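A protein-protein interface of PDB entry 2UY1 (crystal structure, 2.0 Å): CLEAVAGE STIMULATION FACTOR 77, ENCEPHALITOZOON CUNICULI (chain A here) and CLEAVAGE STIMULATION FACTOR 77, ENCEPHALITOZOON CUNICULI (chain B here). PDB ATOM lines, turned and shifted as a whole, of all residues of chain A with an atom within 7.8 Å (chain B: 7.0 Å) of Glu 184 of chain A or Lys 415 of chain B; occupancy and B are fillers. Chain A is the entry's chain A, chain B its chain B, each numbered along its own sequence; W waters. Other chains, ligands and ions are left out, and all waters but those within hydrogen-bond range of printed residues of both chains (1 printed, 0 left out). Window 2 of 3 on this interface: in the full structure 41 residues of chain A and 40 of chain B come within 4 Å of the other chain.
The side-chain carboxylate of Glu 184 of chain A is in salt-bridge range of the side-chain amino group of Lys 415 of chain B (3.1 Å).
NZ of Lys 410 of chain B sits at hydrogen-bond distance from OE1 of Gln 431 of chain A, at 3.1 Å.
O of Gly 434 of chain A lies close to SD of Met 411 of chain B.
Ile 414 of chain B touches Gln 431 of chain A.
OE1 of Gln 431 of chain A touches CD1 of Ile 419 of chain B, at 3.7 Å.
OE1 of Glu 433 of chain A touches CG2 of Ile 414 of chain B, 3.4 Å away.
Met 183 of chain A touches none of the printed residues of chain B.
Glu 184 of chain A touches just one residue of chain B: Lys 415 (3.0 Å).
His 194 of chain A touches none of the printed residues of chain B.
Of the printed residues of chain B, Gly 434 of chain A touches Met 411.
Of the printed residues of chain A, Lys 410 of chain B touches Gln 431.
Printed residues of chain A within 4 Å of Met 411 of chain B: Gly 434 (3.5 Å).
Printed residues of chain A within 4 Å of Ile 414 of chain B: Gln 431 and Glu 433.
Printed residues of chain A within 4 Å of Ile 419 of chain B: Gln 431 (3.7 Å).
The nearest residue of chain A that does not touch Lys 415 of chain B is Glu 433 of chain A (5.4 Å).
Of the 17 printed residues of chain A, 4 touch a printed residue of chain B.
Printed residues of chain A that touch a printed residue of chain B: Glu 184, Gln 431, Glu 433 and Gly 434.
Hydrophobic or aromatic side chains of chain B within 4 Å of the printed part of chain A: Met 411, Ile 414 and Ile 419.
Among the printed residues, 6 pairs touch across the chains.
Water W1 bridges O of Met 411 of chain B (2.7 Å) and N of Gly 434 of chain A (2.8 Å).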
ATOM      1  N   LEU A 178     -16.447  32.118 -18.775  1.00  0.00           N
ATOM      2  CA  LEU A 178     -15.307  32.057 -17.875  1.00  0.00           C
ATOM      3  C   LEU A 178     -15.632  31.100 -16.723  1.00  0.00           C
ATOM      4  O   LEU A 178     -14.776  30.316 -16.303  1.00  0.00           O
ATOM      5  CB  LEU A 178     -14.899  33.455 -17.380  1.00  0.00           C
ATOM      6  CG  LEU A 178     -13.941  33.572 -16.158  1.00  0.00           C
ATOM      7  CD1 LEU A 178     -12.520  33.113 -16.485  1.00  0.00           C
ATOM      8  CD2 LEU A 178     -13.998  35.013 -15.605  1.00  0.00           C
ATOM      9  N   ILE A 179     -16.845  31.185 -16.191  1.00  0.00           N
ATOM     10  CA  ILE A 179     -17.272  30.209 -15.120  1.00  0.00           C
ATOM     11  C   ILE A 179     -17.111  28.749 -15.549  1.00  0.00           C
ATOM     12  O   ILE A 179     -16.496  27.916 -14.848  1.00  0.00           O
ATOM     13  CB  ILE A 179     -18.755  30.489 -14.608  1.00  0.00           C
ATOM     14  CG1 ILE A 179     -18.801  31.819 -13.833  1.00  0.00           C
ATOM     15  CG2 ILE A 179     -19.252  29.293 -13.753  1.00  0.00           C
ATOM     16  CD1 ILE A 179     -20.195  32.421 -13.506  1.00  0.00           C
ATOM     17  N   ASP A 180     -17.595  28.432 -16.745  1.00  0.00           N
ATOM     18  CA  ASP A 180     -17.510  27.055 -17.276  1.00  0.00           C
ATOM     19  C   ASP A 180     -16.070  26.581 -17.433  1.00  0.00           C
ATOM     20  O   ASP A 180     -15.742  25.387 -17.192  1.00  0.00           O
ATOM     21  CB  ASP A 180     -18.212  27.009 -18.656  1.00  0.00           C
ATOM     22  CG  ASP A 180     -19.726  27.344 -18.618  1.00  0.00           C
ATOM     23  OD1 ASP A 180     -20.413  27.085 -17.594  1.00  0.00           O
ATOM     24  OD2 ASP A 180     -20.263  27.807 -19.669  1.00  0.00           O
ATOM     25  N   LEU A 181     -15.176  27.486 -17.888  1.00  0.00           N
ATOM     26  CA  LEU A 181     -13.797  27.114 -18.099  1.00  0.00           C
ATOM     27  C   LEU A 181     -13.058  26.807 -16.767  1.00  0.00           C
ATOM     28  O   LEU A 181     -12.229  25.867 -16.710  1.00  0.00           O
ATOM     29  CB  LEU A 181     -13.086  28.261 -18.904  1.00  0.00           C
ATOM     30  CG  LEU A 181     -11.578  28.398 -18.835  1.00  0.00           C
ATOM     31  CD1 LEU A 181     -10.937  27.215 -19.555  1.00  0.00           C
ATOM     32  CD2 LEU A 181     -11.131  29.726 -19.473  1.00  0.00           C
ATOM     33  N   GLU A 182     -13.355  27.577 -15.730  1.00  0.00           N
ATOM     34  CA  GLU A 182     -12.690  27.440 -14.429  1.00  0.00           C
ATOM     35  C   GLU A 182     -13.281  26.273 -13.633  1.00  0.00           C
ATOM     36  O   GLU A 182     -12.565  25.615 -12.850  1.00  0.00           O
ATOM     37  CB  GLU A 182     -12.817  28.734 -13.635  1.00  0.00           C
ATOM     38  CG  GLU A 182     -11.812  29.857 -14.029  1.00  0.00           C
ATOM     39  CD  GLU A 182     -10.363  29.480 -13.836  1.00  0.00           C
ATOM     40  OE1 GLU A 182     -10.039  28.637 -12.973  1.00  0.00           O
ATOM     41  OE2 GLU A 182      -9.515  30.042 -14.548  1.00  0.00           O
ATOM     42  N   MET A 183     -14.557  25.971 -13.884  1.00  0.00           N
ATOM     43  CA  MET A 183     -15.214  24.724 -13.357  1.00  0.00           C
ATOM     44  C   MET A 183     -14.583  23.422 -13.906  1.00  0.00           C
ATOM     45  O   MET A 183     -14.667  22.332 -13.318  1.00  0.00           O
ATOM     46  CB  MET A 183     -16.734  24.730 -13.674  1.00  0.00           C
ATOM     47  CG  MET A 183     -17.594  25.586 -12.806  1.00  0.00           C
ATOM     48  SD  MET A 183     -17.391  25.159 -11.032  1.00  0.00           S
ATOM     49  CE  MET A 183     -18.596  23.869 -10.864  1.00  0.00           C
ATOM     50  N   GLU A 184     -13.946  23.515 -15.052  1.00  0.00           N
ATOM     51  CA  GLU A 184     -13.304  22.331 -15.598  1.00  0.00           C
ATOM     52  C   GLU A 184     -12.035  21.925 -14.788  1.00  0.00           C
ATOM     53  O   GLU A 184     -11.668  20.734 -14.750  1.00  0.00           O
ATOM     54  CB  GLU A 184     -13.043  22.509 -17.082  1.00  0.00           C
ATOM     55  CG  GLU A 184     -14.301  22.430 -17.968  1.00  0.00           C
ATOM     56  CD  GLU A 184     -14.922  21.027 -17.996  1.00  0.00           C
ATOM     57  OE1 GLU A 184     -14.140  20.049 -18.242  1.00  0.00           O
ATOM     58  OE2 GLU A 184     -16.188  20.912 -17.791  1.00  0.00           O
ATOM     59  N   ASN A 185     -11.413  22.911 -14.111  1.00  0.00           N
ATOM     60  CA  ASN A 185     -10.310  22.699 -13.160  1.00  0.00           C
ATOM     61  C   ASN A 185      -9.094  22.023 -13.813  1.00  0.00           C
ATOM     62  O   ASN A 185      -8.751  20.895 -13.488  1.00  0.00           O
ATOM     63  CB  ASN A 185     -10.817  21.945 -11.913  1.00  0.00           C
ATOM     64  CG  ASN A 185      -9.859  22.025 -10.750  1.00  0.00           C
ATOM     65  OD1 ASN A 185      -8.836  22.726 -10.813  1.00  0.00           O
ATOM     66  ND2 ASN A 185     -10.179  21.308  -9.661  1.00  0.00           N
ATOM     67  N   GLY A 186      -8.467  22.732 -14.755  1.00  0.00           N
ATOM     68  CA  GLY A 186      -7.307  22.228 -15.509  1.00  0.00           C
ATOM     69  C   GLY A 186      -6.014  22.117 -14.708  1.00  0.00           C
ATOM     70  O   GLY A 186      -5.061  21.424 -15.118  1.00  0.00           O
ATOM     71  N   MET A 187      -5.975  22.808 -13.572  1.00  0.00           N
ATOM     72  CA  MET A 187      -4.828  22.791 -12.675  1.00  0.00           C
ATOM     73  C   MET A 187      -5.083  21.838 -11.522  1.00  0.00           C
ATOM     74  O   MET A 187      -4.242  21.685 -10.622  1.00  0.00           O
ATOM     75  CB  MET A 187      -4.569  24.179 -12.144  1.00  0.00           C
ATOM     76  CG  MET A 187      -3.988  25.109 -13.178  1.00  0.00           C
ATOM     77  SD  MET A 187      -2.235  24.762 -13.458  1.00  0.00           S
ATOM     78  CE  MET A 187      -1.520  25.018 -11.822  1.00  0.00           C
ATOM     79  N   LYS A 188      -6.253  21.198 -11.554  1.00  0.00           N
ATOM     80  CA  LYS A 188      -6.563  20.120 -10.626  1.00  0.00           C
ATOM     81  C   LYS A 188      -6.382  20.712  -9.235  1.00  0.00           C
ATOM     82  O   LYS A 188      -5.688  20.136  -8.380  1.00  0.00           O
ATOM     83  CB  LYS A 188      -5.639  18.907 -10.852  1.00  0.00           C
ATOM     84  CG  LYS A 188      -5.616  18.369 -12.280  1.00  0.00           C
ATOM     85  CD  LYS A 188      -5.039  16.943 -12.302  1.00  0.00           C
ATOM     86  CE  LYS A 188      -5.653  16.077 -13.441  1.00  0.00           C
ATOM     87  NZ  LYS A 188      -4.912  14.789 -13.715  1.00  0.00           N
ATOM     88  N   LEU A 189      -6.971  21.895  -9.052  1.00  0.00           N
ATOM     89  CA  LEU A 189      -6.998  22.571  -7.773  1.00  0.00           C
ATOM     90  C   LEU A 189      -7.623  21.644  -6.728  1.00  0.00           C
ATOM     91  O   LEU A 189      -8.635  20.963  -6.989  1.00  0.00           O
ATOM     92  CB  LEU A 189      -7.777  23.899  -7.855  1.00  0.00           C
ATOM     93  CG  LEU A 189      -7.089  25.249  -8.145  1.00  0.00           C
ATOM     94  CD1 LEU A 189      -6.263  25.282  -9.445  1.00  0.00           C
ATOM     95  CD2 LEU A 189      -8.107  26.376  -8.178  1.00  0.00           C
ATOM     96  N   HIS A 194      -9.942  25.514  -5.151  1.00  0.00           N
ATOM     97  CA  HIS A 194     -10.848  25.618  -6.308  1.00  0.00           C
ATOM     98  C   HIS A 194     -12.139  26.373  -5.908  1.00  0.00           C
ATOM     99  O   HIS A 194     -12.557  27.312  -6.588  1.00  0.00           O
ATOM    100  CB  HIS A 194     -11.140  24.259  -6.975  1.00  0.00           C
ATOM    101  CG  HIS A 194     -11.951  24.388  -8.221  1.00  0.00           C
ATOM    102  ND1 HIS A 194     -13.295  24.086  -8.266  1.00  0.00           N
ATOM    103  CD2 HIS A 194     -11.627  24.855  -9.451  1.00  0.00           C
ATOM    104  CE1 HIS A 194     -13.751  24.319  -9.479  1.00  0.00           C
ATOM    105  NE2 HIS A 194     -12.762  24.797 -10.212  1.00  0.00           N
ATOM    106  N   MET A 198     -13.631  29.895  -7.325  1.00  0.00           N
ATOM    107  CA  MET A 198     -14.980  30.061  -7.843  1.00  0.00           C
ATOM    108  C   MET A 198     -15.755  31.135  -7.138  1.00  0.00           C
ATOM    109  O   MET A 198     -16.470  31.883  -7.792  1.00  0.00           O
ATOM    110  CB  MET A 198     -15.737  28.714  -7.846  1.00  0.00           C
ATOM    111  CG  MET A 198     -15.100  27.611  -8.794  1.00  0.00           C
ATOM    112  SD  MET A 198     -14.617  28.103 -10.463  1.00  0.00           S
ATOM    113  CE  MET A 198     -16.194  28.736 -11.066  1.00  0.00           C
ATOM    114  N   GLN A 431     -29.408  27.749 -28.888  1.00  0.00           N
ATOM    115  CA  GLN A 431     -29.057  26.905 -27.764  1.00  0.00           C
ATOM    116  C   GLN A 431     -27.792  27.398 -27.046  1.00  0.00           C
ATOM    117  O   GLN A 431     -26.736  27.542 -27.640  1.00  0.00           O
ATOM    118  CB  GLN A 431     -28.883  25.492 -28.266  1.00  0.00           C
ATOM    119  CG  GLN A 431     -28.028  24.606 -27.419  1.00  0.00           C
ATOM    120  CD  GLN A 431     -27.830  23.277 -28.075  1.00  0.00           C
ATOM    121  OE1 GLN A 431     -28.728  22.346 -27.775  1.00  0.00           O
ATOM    122  NE2 GLN A 431     -26.900  23.080 -28.872  1.00  0.00           N
ATOM    123  N   GLU A 433     -25.041  26.849 -23.747  1.00  0.00           N
ATOM    124  CA  GLU A 433     -24.370  25.731 -23.094  1.00  0.00           C
ATOM    125  C   GLU A 433     -23.833  26.157 -21.742  1.00  0.00           C
ATOM    126  O   GLU A 433     -23.969  27.311 -21.380  1.00  0.00           O
ATOM    127  CB  GLU A 433     -23.248  25.171 -23.971  1.00  0.00           C
ATOM    128  CG  GLU A 433     -22.560  26.163 -24.887  1.00  0.00           C
ATOM    129  CD  GLU A 433     -21.940  25.455 -26.062  1.00  0.00           C
ATOM    130  OE1 GLU A 433     -22.585  25.439 -27.163  1.00  0.00           O
ATOM    131  OE2 GLU A 433     -20.840  24.857 -25.847  1.00  0.00           O
ATOM    132  N   GLY A 434     -23.224  25.230 -21.032  1.00  0.00           N
ATOM    133  CA  GLY A 434     -22.914  25.376 -19.607  1.00  0.00           C
ATOM    134  C   GLY A 434     -23.895  26.173 -18.782  1.00  0.00           C
ATOM    135  O   GLY A 434     -25.120  26.048 -18.950  1.00  0.00           O
ATOM    136  N   LYS B 410     -28.286  17.214 -20.820  1.00  0.00           N
ATOM    137  CA  LYS B 410     -28.219  18.036 -22.009  1.00  0.00           C
ATOM    138  C   LYS B 410     -26.901  18.874 -22.068  1.00  0.00           C
ATOM    139  O   LYS B 410     -26.305  18.961 -23.119  1.00  0.00           O
ATOM    140  CB  LYS B 410     -29.491  18.955 -22.149  1.00  0.00           C
ATOM    141  CG  LYS B 410     -29.707  19.399 -23.545  1.00  0.00           C
ATOM    142  CD  LYS B 410     -30.505  20.677 -23.728  1.00  0.00           C
ATOM    143  CE  LYS B 410     -30.386  21.013 -25.248  1.00  0.00           C
ATOM    144  NZ  LYS B 410     -30.973  22.319 -25.571  1.00  0.00           N
ATOM    145  N   MET B 411     -26.494  19.540 -20.972  1.00  0.00           N
ATOM    146  CA  MET B 411     -25.233  20.356 -20.991  1.00  0.00           C
ATOM    147  C   MET B 411     -23.992  19.523 -21.245  1.00  0.00           C
ATOM    148  O   MET B 411     -23.070  19.999 -21.967  1.00  0.00           O
ATOM    149  CB  MET B 411     -25.045  21.198 -19.716  1.00  0.00           C
ATOM    150  CG  MET B 411     -26.224  22.111 -19.370  1.00  0.00           C
ATOM    151  SD  MET B 411     -26.557  23.308 -20.686  1.00  0.00           S
ATOM    152  CE  MET B 411     -27.900  22.522 -21.574  1.00  0.00           C
ATOM    153  N   ASP B 412     -23.962  18.310 -20.670  1.00  0.00           N
ATOM    154  CA  ASP B 412     -22.951  17.288 -20.958  1.00  0.00           C
ATOM    155  C   ASP B 412     -22.879  16.894 -22.436  1.00  0.00           C
ATOM    156  O   ASP B 412     -21.780  16.746 -22.984  1.00  0.00           O
ATOM    157  CB  ASP B 412     -23.162  16.020 -20.123  1.00  0.00           C
ATOM    158  CG  ASP B 412     -22.918  16.269 -18.629  1.00  0.00           C
ATOM    159  OD1 ASP B 412     -22.260  17.290 -18.322  1.00  0.00           O
ATOM    160  OD2 ASP B 412     -23.443  15.493 -17.778  1.00  0.00           O
ATOM    161  N   ALA B 413     -24.033  16.697 -23.049  1.00  0.00           N
ATOM    162  CA  ALA B 413     -24.139  16.300 -24.439  1.00  0.00           C
ATOM    163  C   ALA B 413     -23.675  17.394 -25.404  1.00  0.00           C
ATOM    164  O   ALA B 413     -23.067  17.070 -26.413  1.00  0.00           O
ATOM    165  CB  ALA B 413     -25.599  15.861 -24.759  1.00  0.00           C
ATOM    166  N   ILE B 414     -24.072  18.661 -25.161  1.00  0.00           N
ATOM    167  CA  ILE B 414     -23.567  19.813 -25.934  1.00  0.00           C
ATOM    168  C   ILE B 414     -22.006  19.810 -25.850  1.00  0.00           C
ATOM    169  O   ILE B 414     -21.294  19.881 -26.886  1.00  0.00           O
ATOM    170  CB  ILE B 414     -24.123  21.155 -25.399  1.00  0.00           C
ATOM    171  CG1 ILE B 414     -25.662  21.240 -25.530  1.00  0.00           C
ATOM    172  CG2 ILE B 414     -23.417  22.364 -26.029  1.00  0.00           C
ATOM    173  CD1 ILE B 414     -26.252  22.426 -24.799  1.00  0.00           C
ATOM    174  N   LYS B 415     -21.502  19.688 -24.627  1.00  0.00           N
ATOM    175  CA  LYS B 415     -20.051  19.694 -24.360  1.00  0.00           C
ATOM    176  C   LYS B 415     -19.311  18.582 -25.126  1.00  0.00           C
ATOM    177  O   LYS B 415     -18.269  18.850 -25.747  1.00  0.00           O
ATOM    178  CB  LYS B 415     -19.782  19.602 -22.859  1.00  0.00           C
ATOM    179  CG  LYS B 415     -18.368  19.917 -22.424  1.00  0.00           C
ATOM    180  CD  LYS B 415     -18.169  19.665 -20.925  1.00  0.00           C
ATOM    181  CE  LYS B 415     -16.731  19.239 -20.629  1.00  0.00           C
ATOM    182  NZ  LYS B 415     -15.775  20.440 -20.790  1.00  0.00           N
ATOM    183  N   ALA B 416     -19.865  17.369 -25.106  1.00  0.00           N
ATOM    184  CA  ALA B 416     -19.303  16.196 -25.820  1.00  0.00           C
ATOM    185  C   ALA B 416     -19.548  16.224 -27.332  1.00  0.00           C
ATOM    186  O   ALA B 416     -19.154  15.300 -28.040  1.00  0.00           O
ATOM    187  CB  ALA B 416     -19.836  14.866 -25.234  1.00  0.00           C
ATOM    188  N   ASP B 417     -20.205  17.273 -27.808  1.00  0.00           N
ATOM    189  CA  ASP B 417     -20.632  17.389 -29.208  1.00  0.00           C
ATOM    190  C   ASP B 417     -21.428  16.154 -29.656  1.00  0.00           C
ATOM    191  O   ASP B 417     -21.346  15.715 -30.804  1.00  0.00           O
ATOM    192  CB  ASP B 417     -19.457  17.805 -30.117  1.00  0.00           C
ATOM    193  CG  ASP B 417     -19.875  18.070 -31.576  1.00  0.00           C
ATOM    194  OD1 ASP B 417     -20.963  18.651 -31.857  1.00  0.00           O
ATOM    195  OD2 ASP B 417     -19.080  17.701 -32.463  1.00  0.00           O
ATOM    196  N   ALA B 418     -22.248  15.636 -28.727  1.00  0.00           N
ATOM    197  CA  ALA B 418     -23.088  14.458 -28.905  1.00  0.00           C
ATOM    198  C   ALA B 418     -24.533  14.720 -29.318  1.00  0.00           C
ATOM    199  O   ALA B 418     -25.325  13.782 -29.397  1.00  0.00           O
ATOM    200  CB  ALA B 418     -23.098  13.642 -27.583  1.00  0.00           C
ATOM    201  N   ILE B 419     -24.942  15.966 -29.513  1.00  0.00           N
ATOM    202  CA  ILE B 419     -26.353  16.169 -29.907  1.00  0.00           C
ATOM    203  C   ILE B 419     -26.497  15.918 -31.404  1.00  0.00           C
ATOM    204  O   ILE B 419     -25.713  16.391 -32.205  1.00  0.00           O
ATOM    205  CB  ILE B 419     -26.870  17.561 -29.551  1.00  0.00           C
ATOM    206  CG1 ILE B 419     -26.856  17.762 -28.009  1.00  0.00           C
ATOM    207  CG2 ILE B 419     -28.209  17.878 -30.286  1.00  0.00           C
ATOM    208  CD1 ILE B 419     -27.805  18.780 -27.462  1.00  0.00           C
HETATM  209  O   HOH W   1     -22.541  22.677 -21.889  1.00  0.00           O
